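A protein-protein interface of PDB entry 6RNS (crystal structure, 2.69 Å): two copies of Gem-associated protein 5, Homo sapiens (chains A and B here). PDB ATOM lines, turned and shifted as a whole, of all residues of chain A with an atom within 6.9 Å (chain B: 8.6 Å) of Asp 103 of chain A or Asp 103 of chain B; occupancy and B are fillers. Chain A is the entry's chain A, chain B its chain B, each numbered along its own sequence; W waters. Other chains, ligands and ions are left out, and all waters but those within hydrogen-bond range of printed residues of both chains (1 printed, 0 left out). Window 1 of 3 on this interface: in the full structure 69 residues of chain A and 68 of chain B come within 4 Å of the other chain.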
ATOM      1  N   LEU A 101      17.322   4.508 -16.838  1.00  0.00           N
ATOM      2  CA  LEU A 101      17.821   3.570 -15.842  1.00  0.00           C
ATOM      3  C   LEU A 101      17.791   2.146 -16.388  1.00  0.00           C
ATOM      4  O   LEU A 101      17.005   1.810 -17.277  1.00  0.00           O
ATOM      5  CB  LEU A 101      16.995   3.656 -14.561  1.00  0.00           C
ATOM      6  CG  LEU A 101      17.079   4.977 -13.804  1.00  0.00           C
ATOM      7  CD1 LEU A 101      16.086   5.016 -12.656  1.00  0.00           C
ATOM      8  CD2 LEU A 101      18.488   5.206 -13.285  1.00  0.00           C
ATOM      9  N   THR A 102      18.662   1.305 -15.835  1.00  0.00           N
ATOM     10  CA  THR A 102      18.827  -0.063 -16.298  1.00  0.00           C
ATOM     11  C   THR A 102      19.109  -0.956 -15.099  1.00  0.00           C
ATOM     12  O   THR A 102      19.403  -0.482 -13.998  1.00  0.00           O
ATOM     13  CB  THR A 102      19.971  -0.189 -17.320  1.00  0.00           C
ATOM     14  OG1 THR A 102      21.216   0.175 -16.702  1.00  0.00           O
ATOM     15  CG2 THR A 102      19.727   0.708 -18.532  1.00  0.00           C
ATOM     16  N   ASP A 103      19.013  -2.268 -15.321  1.00  0.00           N
ATOM     17  CA  ASP A 103      19.462  -3.218 -14.310  1.00  0.00           C
ATOM     18  C   ASP A 103      20.945  -3.040 -14.034  1.00  0.00           C
ATOM     19  O   ASP A 103      21.384  -3.087 -12.879  1.00  0.00           O
ATOM     20  CB  ASP A 103      19.183  -4.646 -14.771  1.00  0.00           C
ATOM     21  CG  ASP A 103      17.722  -4.895 -15.024  1.00  0.00           C
ATOM     22  OD1 ASP A 103      16.904  -4.523 -14.156  1.00  0.00           O
ATOM     23  OD2 ASP A 103      17.388  -5.449 -16.092  1.00  0.00           O
ATOM     24  N   ASN A 104      21.734  -2.845 -15.092  1.00  0.00           N
ATOM     25  CA  ASN A 104      23.161  -2.591 -14.946  1.00  0.00           C
ATOM     26  C   ASN A 104      23.417  -1.444 -13.975  1.00  0.00           C
ATOM     27  O   ASN A 104      24.247  -1.561 -13.067  1.00  0.00           O
ATOM     28  CB  ASN A 104      23.754  -2.288 -16.324  1.00  0.00           C
ATOM     29  CG  ASN A 104      25.243  -2.053 -16.283  1.00  0.00           C
ATOM     30  OD1 ASN A 104      25.981  -2.782 -15.622  1.00  0.00           O
ATOM     31  ND2 ASN A 104      25.695  -1.024 -16.991  1.00  0.00           N
ATOM     32  N   LEU A 105      22.695  -0.331 -14.141  1.00  0.00           N
ATOM     33  CA  LEU A 105      22.915   0.835 -13.288  1.00  0.00           C
ATOM     34  C   LEU A 105      22.536   0.554 -11.839  1.00  0.00           C
ATOM     35  O   LEU A 105      23.211   1.025 -10.916  1.00  0.00           O
ATOM     36  CB  LEU A 105      22.117   2.027 -13.816  1.00  0.00           C
ATOM     37  CG  LEU A 105      22.815   2.934 -14.827  1.00  0.00           C
ATOM     38  CD1 LEU A 105      21.819   3.918 -15.431  1.00  0.00           C
ATOM     39  CD2 LEU A 105      23.982   3.679 -14.187  1.00  0.00           C
ATOM     40  N   VAL A 106      21.449  -0.192 -11.616  1.00  0.00           N
ATOM     41  CA  VAL A 106      21.042  -0.520 -10.255  1.00  0.00           C
ATOM     42  C   VAL A 106      21.991  -1.542  -9.641  1.00  0.00           C
ATOM     43  O   VAL A 106      22.196  -1.553  -8.420  1.00  0.00           O
ATOM     44  CB  VAL A 106      19.588  -1.031 -10.238  1.00  0.00           C
ATOM     45  CG1 VAL A 106      19.166  -1.405  -8.823  1.00  0.00           C
ATOM     46  CG2 VAL A 106      18.651   0.011 -10.817  1.00  0.00           C
ATOM     47  N   ALA A 107      22.575  -2.420 -10.461  1.00  0.00           N
ATOM     48  CA  ALA A 107      23.518  -3.403  -9.939  1.00  0.00           C
ATOM     49  C   ALA A 107      24.784  -2.740  -9.408  1.00  0.00           C
ATOM     50  O   ALA A 107      25.435  -3.287  -8.511  1.00  0.00           O
ATOM     51  CB  ALA A 107      23.873  -4.421 -11.023  1.00  0.00           C
ATOM     52  N   MET A 108      25.147  -1.572  -9.943  1.00  0.00           N
ATOM     53  CA  MET A 108      26.328  -0.848  -9.497  1.00  0.00           C
ATOM     54  C   MET A 108      26.012   0.273  -8.517  1.00  0.00           C
ATOM     55  O   MET A 108      26.938   0.827  -7.918  1.00  0.00           O
ATOM     56  CB  MET A 108      27.075  -0.252 -10.697  1.00  0.00           C
ATOM     57  CG  MET A 108      27.529  -1.272 -11.721  1.00  0.00           C
ATOM     58  SD  MET A 108      28.428  -0.526 -13.095  1.00  0.00           S
ATOM     59  CE  MET A 108      27.157   0.505 -13.830  1.00  0.00           C
ATOM     60  N   ALA A 109      24.741   0.622  -8.345  1.00  0.00           N
ATOM     61  CA  ALA A 109      24.384   1.742  -7.482  1.00  0.00           C
ATOM     62  C   ALA A 109      24.959   1.646  -6.075  1.00  0.00           C
ATOM     63  O   ALA A 109      25.361   2.687  -5.531  1.00  0.00           O
ATOM     64  CB  ALA A 109      22.854   1.869  -7.422  1.00  0.00           C
ATOM     65  N   PHE A 124      13.857   3.361 -10.473  1.00  0.00           N
ATOM     66  CA  PHE A 124      13.742   2.364 -11.533  1.00  0.00           C
ATOM     67  C   PHE A 124      12.358   1.727 -11.549  1.00  0.00           C
ATOM     68  O   PHE A 124      11.850   1.378 -12.622  1.00  0.00           O
ATOM     69  CB  PHE A 124      14.818   1.294 -11.355  1.00  0.00           C
ATOM     70  CG  PHE A 124      14.978   0.374 -12.541  1.00  0.00           C
ATOM     71  CD1 PHE A 124      14.668   0.797 -13.823  1.00  0.00           C
ATOM     72  CD2 PHE A 124      15.450  -0.917 -12.365  1.00  0.00           C
ATOM     73  CE1 PHE A 124      14.825  -0.047 -14.904  1.00  0.00           C
ATOM     74  CE2 PHE A 124      15.605  -1.768 -13.442  1.00  0.00           C
ATOM     75  CZ  PHE A 124      15.291  -1.333 -14.713  1.00  0.00           C
ATOM     76  N   LEU A 128       9.745   1.806 -14.595  1.00  0.00           N
ATOM     77  CA  LEU A 128       9.202   0.593 -15.193  1.00  0.00           C
ATOM     78  C   LEU A 128       7.683   0.650 -15.304  1.00  0.00           C
ATOM     79  O   LEU A 128       7.109   0.091 -16.246  1.00  0.00           O
ATOM     80  CB  LEU A 128       9.638  -0.625 -14.380  1.00  0.00           C
ATOM     81  CG  LEU A 128      11.105  -1.026 -14.526  1.00  0.00           C
ATOM     82  CD1 LEU A 128      11.485  -2.070 -13.486  1.00  0.00           C
ATOM     83  CD2 LEU A 128      11.382  -1.545 -15.932  1.00  0.00           C
ATOM     84  N   LYS A 136       7.869  -6.641 -13.274  1.00  0.00           N
ATOM     85  CA  LYS A 136       9.250  -6.291 -12.967  1.00  0.00           C
ATOM     86  C   LYS A 136       9.299  -5.171 -11.937  1.00  0.00           C
ATOM     87  O   LYS A 136      10.051  -5.244 -10.958  1.00  0.00           O
ATOM     88  CB  LYS A 136       9.982  -5.889 -14.246  1.00  0.00           C
ATOM     89  CG  LYS A 136      11.487  -5.732 -14.090  1.00  0.00           C
ATOM     90  CD  LYS A 136      12.170  -5.661 -15.452  1.00  0.00           C
ATOM     91  CE  LYS A 136      13.657  -5.378 -15.324  1.00  0.00           C
ATOM     92  NZ  LYS A 136      14.222  -4.921 -16.624  1.00  0.00           N
ATOM     93  N   HIS A 140      11.131  -5.469  -8.149  1.00  0.00           N
ATOM     94  CA  HIS A 140      12.147  -4.578  -7.598  1.00  0.00           C
ATOM     95  C   HIS A 140      11.686  -3.929  -6.300  1.00  0.00           C
ATOM     96  O   HIS A 140      12.517  -3.605  -5.443  1.00  0.00           O
ATOM     97  CB  HIS A 140      12.517  -3.509  -8.623  1.00  0.00           C
ATOM     98  CG  HIS A 140      13.432  -4.001  -9.700  1.00  0.00           C
ATOM     99  ND1 HIS A 140      14.742  -4.348  -9.456  1.00  0.00           N
ATOM    100  CD2 HIS A 140      13.229  -4.199 -11.023  1.00  0.00           C
ATOM    101  CE1 HIS A 140      15.308  -4.741 -10.584  1.00  0.00           C
ATOM    102  NE2 HIS A 140      14.410  -4.663 -11.549  1.00  0.00           N
ATOM    103  N   GLN B  80      13.480 -14.942 -11.758  1.00  0.00           N
ATOM    104  CA  GLN B  80      12.544 -13.906 -11.337  1.00  0.00           C
ATOM    105  C   GLN B  80      11.401 -14.486 -10.513  1.00  0.00           C
ATOM    106  O   GLN B  80      10.832 -13.789  -9.664  1.00  0.00           O
ATOM    107  CB  GLN B  80      12.004 -13.170 -12.562  1.00  0.00           C
ATOM    108  CG  GLN B  80      13.075 -12.447 -13.362  1.00  0.00           C
ATOM    109  CD  GLN B  80      12.737 -12.339 -14.838  1.00  0.00           C
ATOM    110  OE1 GLN B  80      13.618 -12.428 -15.694  1.00  0.00           O
ATOM    111  NE2 GLN B  80      11.459 -12.147 -15.142  1.00  0.00           N
ATOM    112  N   LEU B  92      20.618 -16.650  -5.741  1.00  0.00           N
ATOM    113  CA  LEU B  92      21.911 -16.152  -6.199  1.00  0.00           C
ATOM    114  C   LEU B  92      22.954 -17.265  -6.205  1.00  0.00           C
ATOM    115  O   LEU B  92      23.723 -17.404  -7.162  1.00  0.00           O
ATOM    116  CB  LEU B  92      22.372 -14.995  -5.312  1.00  0.00           C
ATOM    117  CG  LEU B  92      21.530 -13.722  -5.352  1.00  0.00           C
ATOM    118  CD1 LEU B  92      21.995 -12.747  -4.280  1.00  0.00           C
ATOM    119  CD2 LEU B  92      21.584 -13.070  -6.724  1.00  0.00           C
ATOM    120  N   GLU B 100      24.247 -18.274 -14.727  1.00  0.00           N
ATOM    121  CA  GLU B 100      23.125 -17.501 -15.238  1.00  0.00           C
ATOM    122  C   GLU B 100      22.967 -16.160 -14.530  1.00  0.00           C
ATOM    123  O   GLU B 100      21.941 -15.496 -14.711  1.00  0.00           O
ATOM    124  CB  GLU B 100      21.832 -18.311 -15.119  1.00  0.00           C
ATOM    125  CG  GLU B 100      21.807 -19.588 -15.953  1.00  0.00           C
ATOM    126  CD  GLU B 100      21.632 -19.320 -17.435  1.00  0.00           C
ATOM    127  OE1 GLU B 100      21.652 -18.136 -17.837  1.00  0.00           O
ATOM    128  OE2 GLU B 100      21.470 -20.295 -18.201  1.00  0.00           O
ATOM    129  N   LEU B 101      23.950 -15.747 -13.727  1.00  0.00           N
ATOM    130  CA  LEU B 101      23.896 -14.441 -13.086  1.00  0.00           C
ATOM    131  C   LEU B 101      23.705 -13.351 -14.133  1.00  0.00           C
ATOM    132  O   LEU B 101      24.177 -13.460 -15.269  1.00  0.00           O
ATOM    133  CB  LEU B 101      25.172 -14.185 -12.283  1.00  0.00           C
ATOM    134  CG  LEU B 101      25.232 -14.781 -10.875  1.00  0.00           C
ATOM    135  CD1 LEU B 101      26.616 -14.576 -10.257  1.00  0.00           C
ATOM    136  CD2 LEU B 101      24.145 -14.190  -9.982  1.00  0.00           C
ATOM    137  N   THR B 102      22.995 -12.293 -13.742  1.00  0.00           N
ATOM    138  CA  THR B 102      22.685 -11.195 -14.643  1.00  0.00           C
ATOM    139  C   THR B 102      22.697  -9.882 -13.869  1.00  0.00           C
ATOM    140  O   THR B 102      22.791  -9.860 -12.640  1.00  0.00           O
ATOM    141  CB  THR B 102      21.314 -11.370 -15.312  1.00  0.00           C
ATOM    142  OG1 THR B 102      20.281 -11.192 -14.333  1.00  0.00           O
ATOM    143  CG2 THR B 102      21.188 -12.749 -15.930  1.00  0.00           C
ATOM    144  N   ASP B 103      22.588  -8.777 -14.610  1.00  0.00           N
ATOM    145  CA  ASP B 103      22.475  -7.469 -13.976  1.00  0.00           C
ATOM    146  C   ASP B 103      21.238  -7.403 -13.089  1.00  0.00           C
ATOM    147  O   ASP B 103      21.309  -6.980 -11.929  1.00  0.00           O
ATOM    148  CB  ASP B 103      22.432  -6.371 -15.040  1.00  0.00           C
ATOM    149  CG  ASP B 103      23.778  -6.149 -15.705  1.00  0.00           C
ATOM    150  OD1 ASP B 103      24.810  -6.270 -15.011  1.00  0.00           O
ATOM    151  OD2 ASP B 103      23.804  -5.853 -16.921  1.00  0.00           O
ATOM    152  N   ASN B 104      20.088  -7.829 -13.621  1.00  0.00           N
ATOM    153  CA  ASN B 104      18.851  -7.796 -12.850  1.00  0.00           C
ATOM    154  C   ASN B 104      18.986  -8.577 -11.549  1.00  0.00           C
ATOM    155  O   ASN B 104      18.504  -8.138 -10.499  1.00  0.00           O
ATOM    156  CB  ASN B 104      17.700  -8.351 -13.687  1.00  0.00           C
ATOM    157  CG  ASN B 104      16.395  -8.400 -12.922  1.00  0.00           C
ATOM    158  OD1 ASN B 104      15.681  -7.400 -12.826  1.00  0.00           O
ATOM    159  ND2 ASN B 104      16.074  -9.568 -12.374  1.00  0.00           N
ATOM    160  N   LEU B 105      19.638  -9.740 -11.596  1.00  0.00           N
ATOM    161  CA  LEU B 105      19.833 -10.521 -10.381  1.00  0.00           C
ATOM    162  C   LEU B 105      20.734  -9.788  -9.394  1.00  0.00           C
ATOM    163  O   LEU B 105      20.452  -9.762  -8.189  1.00  0.00           O
ATOM    164  CB  LEU B 105      20.412 -11.890 -10.727  1.00  0.00           C
ATOM    165  CG  LEU B 105      19.438 -13.069 -10.700  1.00  0.00           C
ATOM    166  CD1 LEU B 105      20.146 -14.348 -11.122  1.00  0.00           C
ATOM    167  CD2 LEU B 105      18.823 -13.214  -9.316  1.00  0.00           C
ATOM    168  N   VAL B 106      21.820  -9.180  -9.881  1.00  0.00           N
ATOM    169  CA  VAL B 106      22.717  -8.450  -8.993  1.00  0.00           C
ATOM    170  C   VAL B 106      22.048  -7.189  -8.464  1.00  0.00           C
ATOM    171  O   VAL B 106      22.299  -6.777  -7.324  1.00  0.00           O
ATOM    172  CB  VAL B 106      24.037  -8.129  -9.720  1.00  0.00           C
ATOM    173  CG1 VAL B 106      24.928  -7.235  -8.862  1.00  0.00           C
ATOM    174  CG2 VAL B 106      24.757  -9.420 -10.087  1.00  0.00           C
ATOM    175  N   ALA B 107      21.186  -6.560  -9.264  1.00  0.00           N
ATOM    176  CA  ALA B 107      20.478  -5.373  -8.794  1.00  0.00           C
ATOM    177  C   ALA B 107      19.699  -5.669  -7.516  1.00  0.00           C
ATOM    178  O   ALA B 107      19.602  -4.817  -6.627  1.00  0.00           O
ATOM    179  CB  ALA B 107      19.547  -4.851  -9.886  1.00  0.00           C
ATOM    180  N   MET B 108      19.129  -6.878  -7.402  1.00  0.00           N
ATOM    181  CA  MET B 108      18.333  -7.253  -6.237  1.00  0.00           C
ATOM    182  C   MET B 108      19.153  -7.887  -5.121  1.00  0.00           C
ATOM    183  O   MET B 108      18.628  -8.069  -4.018  1.00  0.00           O
ATOM    184  CB  MET B 108      17.223  -8.227  -6.649  1.00  0.00           C
ATOM    185  CG  MET B 108      16.139  -7.608  -7.508  1.00  0.00           C
ATOM    186  SD  MET B 108      15.411  -8.800  -8.643  1.00  0.00           S
ATOM    187  CE  MET B 108      14.082  -7.827  -9.345  1.00  0.00           C
ATOM    188  N   ALA B 109      20.415  -8.223  -5.376  1.00  0.00           N
ATOM    189  CA  ALA B 109      21.236  -8.849  -4.348  1.00  0.00           C
ATOM    190  C   ALA B 109      21.353  -8.020  -3.074  1.00  0.00           C
ATOM    191  O   ALA B 109      21.380  -8.617  -1.985  1.00  0.00           O
ATOM    192  CB  ALA B 109      22.632  -9.146  -4.915  1.00  0.00           C
ATOM    193  N   PRO B 110      21.447  -6.685  -3.120  1.00  0.00           N
ATOM    194  CA  PRO B 110      21.577  -5.923  -1.863  1.00  0.00           C
ATOM    195  C   PRO B 110      20.399  -6.094  -0.919  1.00  0.00           C
ATOM    196  O   PRO B 110      20.494  -5.672   0.242  1.00  0.00           O
ATOM    197  CB  PRO B 110      21.706  -4.466  -2.335  1.00  0.00           C
ATOM    198  CG  PRO B 110      22.196  -4.560  -3.744  1.00  0.00           C
ATOM    199  CD  PRO B 110      21.579  -5.819  -4.307  1.00  0.00           C
ATOM    200  N   TRP B 117      25.649  -8.507  -1.709  1.00  0.00           N
ATOM    201  CA  TRP B 117      25.902  -7.812  -2.965  1.00  0.00           C
ATOM    202  C   TRP B 117      27.374  -7.903  -3.350  1.00  0.00           C
ATOM    203  O   TRP B 117      27.713  -8.155  -4.512  1.00  0.00           O
ATOM    204  CB  TRP B 117      25.473  -6.353  -2.858  1.00  0.00           C
ATOM    205  CG  TRP B 117      25.835  -5.552  -4.066  1.00  0.00           C
ATOM    206  CD1 TRP B 117      25.262  -5.631  -5.301  1.00  0.00           C
ATOM    207  CD2 TRP B 117      26.850  -4.549  -4.157  1.00  0.00           C
ATOM    208  NE1 TRP B 117      25.856  -4.738  -6.156  1.00  0.00           N
ATOM    209  CE2 TRP B 117      26.834  -4.061  -5.478  1.00  0.00           C
ATOM    210  CE3 TRP B 117      27.770  -4.014  -3.251  1.00  0.00           C
ATOM    211  CZ2 TRP B 117      27.705  -3.065  -5.915  1.00  0.00           C
ATOM    212  CZ3 TRP B 117      28.632  -3.027  -3.685  1.00  0.00           C
ATOM    213  CH2 TRP B 117      28.593  -2.564  -5.006  1.00  0.00           C
ATOM    214  N   ALA B 120      27.967 -11.132  -4.771  1.00  0.00           N
ATOM    215  CA  ALA B 120      27.320 -11.309  -6.066  1.00  0.00           C
ATOM    216  C   ALA B 120      28.113 -10.641  -7.183  1.00  0.00           C
ATOM    217  O   ALA B 120      28.284 -11.222  -8.260  1.00  0.00           O
ATOM    218  CB  ALA B 120      25.894 -10.757  -6.019  1.00  0.00           C
ATOM    219  N   VAL B 121      28.606  -9.422  -6.945  1.00  0.00           N
ATOM    220  CA  VAL B 121      29.351  -8.705  -7.977  1.00  0.00           C
ATOM    221  C   VAL B 121      30.623  -9.462  -8.341  1.00  0.00           C
ATOM    222  O   VAL B 121      30.944  -9.641  -9.522  1.00  0.00           O
ATOM    223  CB  VAL B 121      29.660  -7.271  -7.515  1.00  0.00           C
ATOM    224  CG1 VAL B 121      30.775  -6.673  -8.355  1.00  0.00           C
ATOM    225  CG2 VAL B 121      28.415  -6.408  -7.602  1.00  0.00           C
ATOM    226  N   PHE B 124      29.448 -12.451 -10.295  1.00  0.00           N
ATOM    227  CA  PHE B 124      29.080 -12.013 -11.639  1.00  0.00           C
ATOM    228  C   PHE B 124      30.306 -11.572 -12.429  1.00  0.00           C
ATOM    229  O   PHE B 124      30.335 -11.713 -13.657  1.00  0.00           O
ATOM    230  CB  PHE B 124      28.054 -10.881 -11.549  1.00  0.00           C
ATOM    231  CG  PHE B 124      27.425 -10.509 -12.870  1.00  0.00           C
ATOM    232  CD1 PHE B 124      27.308 -11.436 -13.892  1.00  0.00           C
ATOM    233  CD2 PHE B 124      26.952  -9.223 -13.085  1.00  0.00           C
ATOM    234  CE1 PHE B 124      26.729 -11.090 -15.102  1.00  0.00           C
ATOM    235  CE2 PHE B 124      26.376  -8.869 -14.293  1.00  0.00           C
ATOM    236  CZ  PHE B 124      26.264  -9.804 -15.302  1.00  0.00           C
ATOM    237  N   GLN B 127      32.273 -14.752 -13.589  1.00  0.00           N
ATOM    238  CA  GLN B 127      31.491 -15.344 -14.667  1.00  0.00           C
ATOM    239  C   GLN B 127      31.589 -14.524 -15.946  1.00  0.00           C
ATOM    240  O   GLN B 127      31.634 -15.084 -17.047  1.00  0.00           O
ATOM    241  CB  GLN B 127      30.038 -15.470 -14.217  1.00  0.00           C
ATOM    242  CG  GLN B 127      29.046 -15.742 -15.315  1.00  0.00           C
ATOM    243  CD  GLN B 127      27.635 -15.747 -14.782  1.00  0.00           C
ATOM    244  OE1 GLN B 127      27.374 -16.275 -13.701  1.00  0.00           O
ATOM    245  NE2 GLN B 127      26.719 -15.135 -15.522  1.00  0.00           N
ATOM    246  N   LEU B 128      31.604 -13.194 -15.825  1.00  0.00           N
ATOM    247  CA  LEU B 128      31.682 -12.349 -17.010  1.00  0.00           C
ATOM    248  C   LEU B 128      33.023 -12.495 -17.718  1.00  0.00           C
ATOM    249  O   LEU B 128      33.097 -12.313 -18.939  1.00  0.00           O
ATOM    250  CB  LEU B 128      31.438 -10.891 -16.627  1.00  0.00           C
ATOM    251  CG  LEU B 128      29.974 -10.454 -16.609  1.00  0.00           C
ATOM    252  CD1 LEU B 128      29.829  -9.103 -15.928  1.00  0.00           C
ATOM    253  CD2 LEU B 128      29.419 -10.403 -18.027  1.00  0.00           C
ATOM    254  N   GLN B 133      33.697 -10.910 -21.627  1.00  0.00           N
ATOM    255  CA  GLN B 133      33.239  -9.528 -21.451  1.00  0.00           C
ATOM    256  C   GLN B 133      34.095  -8.886 -20.351  1.00  0.00           C
ATOM    257  O   GLN B 133      33.631  -8.552 -19.260  1.00  0.00           O
ATOM    258  CB  GLN B 133      31.746  -9.469 -21.119  1.00  0.00           C
ATOM    259  CG  GLN B 133      30.855 -10.009 -22.224  1.00  0.00           C
ATOM    260  CD  GLN B 133      29.518  -9.299 -22.298  1.00  0.00           C
ATOM    261  OE1 GLN B 133      29.302  -8.448 -23.161  1.00  0.00           O
ATOM    262  NE2 GLN B 133      28.611  -9.647 -21.392  1.00  0.00           N
ATOM    263  N   LYS B 136      33.126  -5.180 -19.227  1.00  0.00           N
ATOM    264  CA  LYS B 136      31.977  -5.172 -18.328  1.00  0.00           C
ATOM    265  C   LYS B 136      32.363  -5.686 -16.946  1.00  0.00           C
ATOM    266  O   LYS B 136      31.968  -5.108 -15.926  1.00  0.00           O
ATOM    267  CB  LYS B 136      30.845  -6.016 -18.913  1.00  0.00           C
ATOM    268  CG  LYS B 136      29.554  -5.962 -18.107  1.00  0.00           C
ATOM    269  CD  LYS B 136      28.467  -6.834 -18.719  1.00  0.00           C
ATOM    270  CE  LYS B 136      27.112  -6.556 -18.081  1.00  0.00           C
ATOM    271  NZ  LYS B 136      26.615  -5.185 -18.398  1.00  0.00           N
ATOM    272  N   ALA B 137      33.138  -6.774 -16.892  1.00  0.00           N
ATOM    273  CA  ALA B 137      33.624  -7.274 -15.611  1.00  0.00           C
ATOM    274  C   ALA B 137      34.477  -6.229 -14.900  1.00  0.00           C
ATOM    275  O   ALA B 137      34.431  -6.110 -13.670  1.00  0.00           O
ATOM    276  CB  ALA B 137      34.422  -8.560 -15.824  1.00  0.00           C
ATOM    277  N   HIS B 140      32.273  -3.797 -13.066  1.00  0.00           N
ATOM    278  CA  HIS B 140      31.654  -4.335 -11.856  1.00  0.00           C
ATOM    279  C   HIS B 140      32.663  -4.424 -10.716  1.00  0.00           C
ATOM    280  O   HIS B 140      32.312  -4.214  -9.550  1.00  0.00           O
ATOM    281  CB  HIS B 140      31.029  -5.699 -12.145  1.00  0.00           C
ATOM    282  CG  HIS B 140      29.754  -5.614 -12.922  1.00  0.00           C
ATOM    283  ND1 HIS B 140      28.575  -5.172 -12.362  1.00  0.00           N
ATOM    284  CD2 HIS B 140      29.480  -5.884 -14.219  1.00  0.00           C
ATOM    285  CE1 HIS B 140      27.625  -5.181 -13.281  1.00  0.00           C
ATOM    286  NE2 HIS B 140      28.149  -5.610 -14.416  1.00  0.00           N
HETATM  287  O   HOH W   1      16.382  -4.193  -7.201  1.00  0.00           O
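The side-chain carboxylate (OD1) of Asp 103 of chain A lies close to the side-chain amide oxygen (OD1) of Asn 104 of chain B, at 3.4 Å. NE1 of Trp 117 of chain B is in hydrogen-bond range of O of Ala 107 of chain A (2.8 Å). A ring nitrogen (NE2) of His 140 of chain A sits at hydrogen-bond distance from the side-chain amide oxygen (OD1) of Asn 104 of chain B, 3.3 Å away.
The backbone NH (N) of Asn 104 of chain A sits close to the side-chain hydroxyl (OG1) of Thr 102 of chain A, 3.5 Å away. The side-chain amino group (NZ) of Lys 136 of chain A lies within salt-bridge range of the side-chain carboxylate (OD2) of Asp 103 of chain A, at 3.3 Å. The side-chain hydroxyl (OG1) of Thr 102 of chain B sits close to the backbone NH (N) of Asn 104 of chain B (3.4 Å). OD2 of Asp 103 of chain B is in salt-bridge range of NZ of Lys 136 of chain B (3.2 Å). The side-chain carboxylate (OD1) of Asp 103 of chain B sits at hydrogen-bond distance from a ring nitrogen (NE2) of His 140 of chain B, 3.5 Å away.
Asp 103 of chain B touches Asp 103 of chain A (CB to CB, 3.7 Å). CB of Ala 107 of chain B touches O of Asp 103 of chain A, at 3.9 Å. N of Asn 104 of chain A touches CB of Asp 103 of chain B, at 3.6 Å. NZ of Lys 136 of chain B touches OD1 of Asn 104 of chain A, 3.7 Å away. CE1 of His 140 of chain B touches OD1 of Asn 104 of chain A, 3.7 Å away. Val 106 of chain A touches Ala 107 of chain B. CB of Ala 107 of chain A touches O of Asp 103 of chain B, 3.7 Å away. CB of Ala 107 of chain A touches CG1 of Val 106 of chain B, 3.7 Å away. Ala 107 of chain A touches Ala 107 of chain B. Lys 136 of chain A touches Asn 104 of chain B.
Asp 103 of chain A touches just these residues of chain B: Asp 103, Asn 104 and Ala 107. Asp 103 of chain B touches three residues of chain A. No residue of chain B comes within 4 Å of Thr 102 of chain A. Of the printed residues of chain A, Met 108 of chain B touches His 140 (3.5 Å). Of the printed residues of chain A, Ala 107 of chain B touches Asp 103 (3.9 Å), Val 106 (3.6 Å) and Ala 107 (3.8 Å). Of the printed residues of chain A, Lys 136 of chain B touches Asn 104. Printed residues of chain B within 4 Å of His 140 of chain A: Asn 104 (3.3 Å) and Met 108 (3.5 Å). Of the printed residues of chain A, His 140 of chain B touches Asn 104 (3.7 Å). Leu 128 of chain B touches none of the printed residues of chain A. Leu 105 of chain B touches none of the printed residues of chain A. The nearest residue of chain B that does not touch Asp 103 of chain A is Leu 105 of chain B (6.0 Å). The nearest printed residue of chain A that does not touch Val 106 of chain B is Val 106 of chain A (5.3 Å).
Of the 13 printed residues of chain A, 6 touch a printed residue of chain B. Hydrophobic or aromatic side chains of chain A that line the printed part of chain B: Val 106, Ala 107 and His 140. Hydrophobic or aromatic side chains of chain B within 4 Å of the printed part of chain A: Val 106, Ala 107, Met 108, Trp 117 and His 140. Among the printed residues, no Asp or Glu carboxylate lies within 4 Å of a Lys or Arg side-chain nitrogen of the other chain.
Asp 103 of chain B touches its own counterpart, Asp 103 of chain A. Asn 104 of chain A touches Lys 136 of chain B, and with the chains exchanged Lys 136 of chain A touches Asn 104 of chain B. Val 106 of chain A touches Ala 107 of chain B, and with the chains exchanged Ala 107 of chain A touches Val 106 of chain B. His 140 of chain A touches Met 108 of chain B, but with the chains exchanged Met 108 of chain A does not touch His 140 of chain B (4.1 Å). Of the 14 pairs that touch across the chains among the printed residues, 12 have their exchanged pair printed and touching as well.
Water W1 bridges a ring nitrogen (ND1) of His 140 of chain A and the backbone carbonyl oxygen of Ala 107 of chain B.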
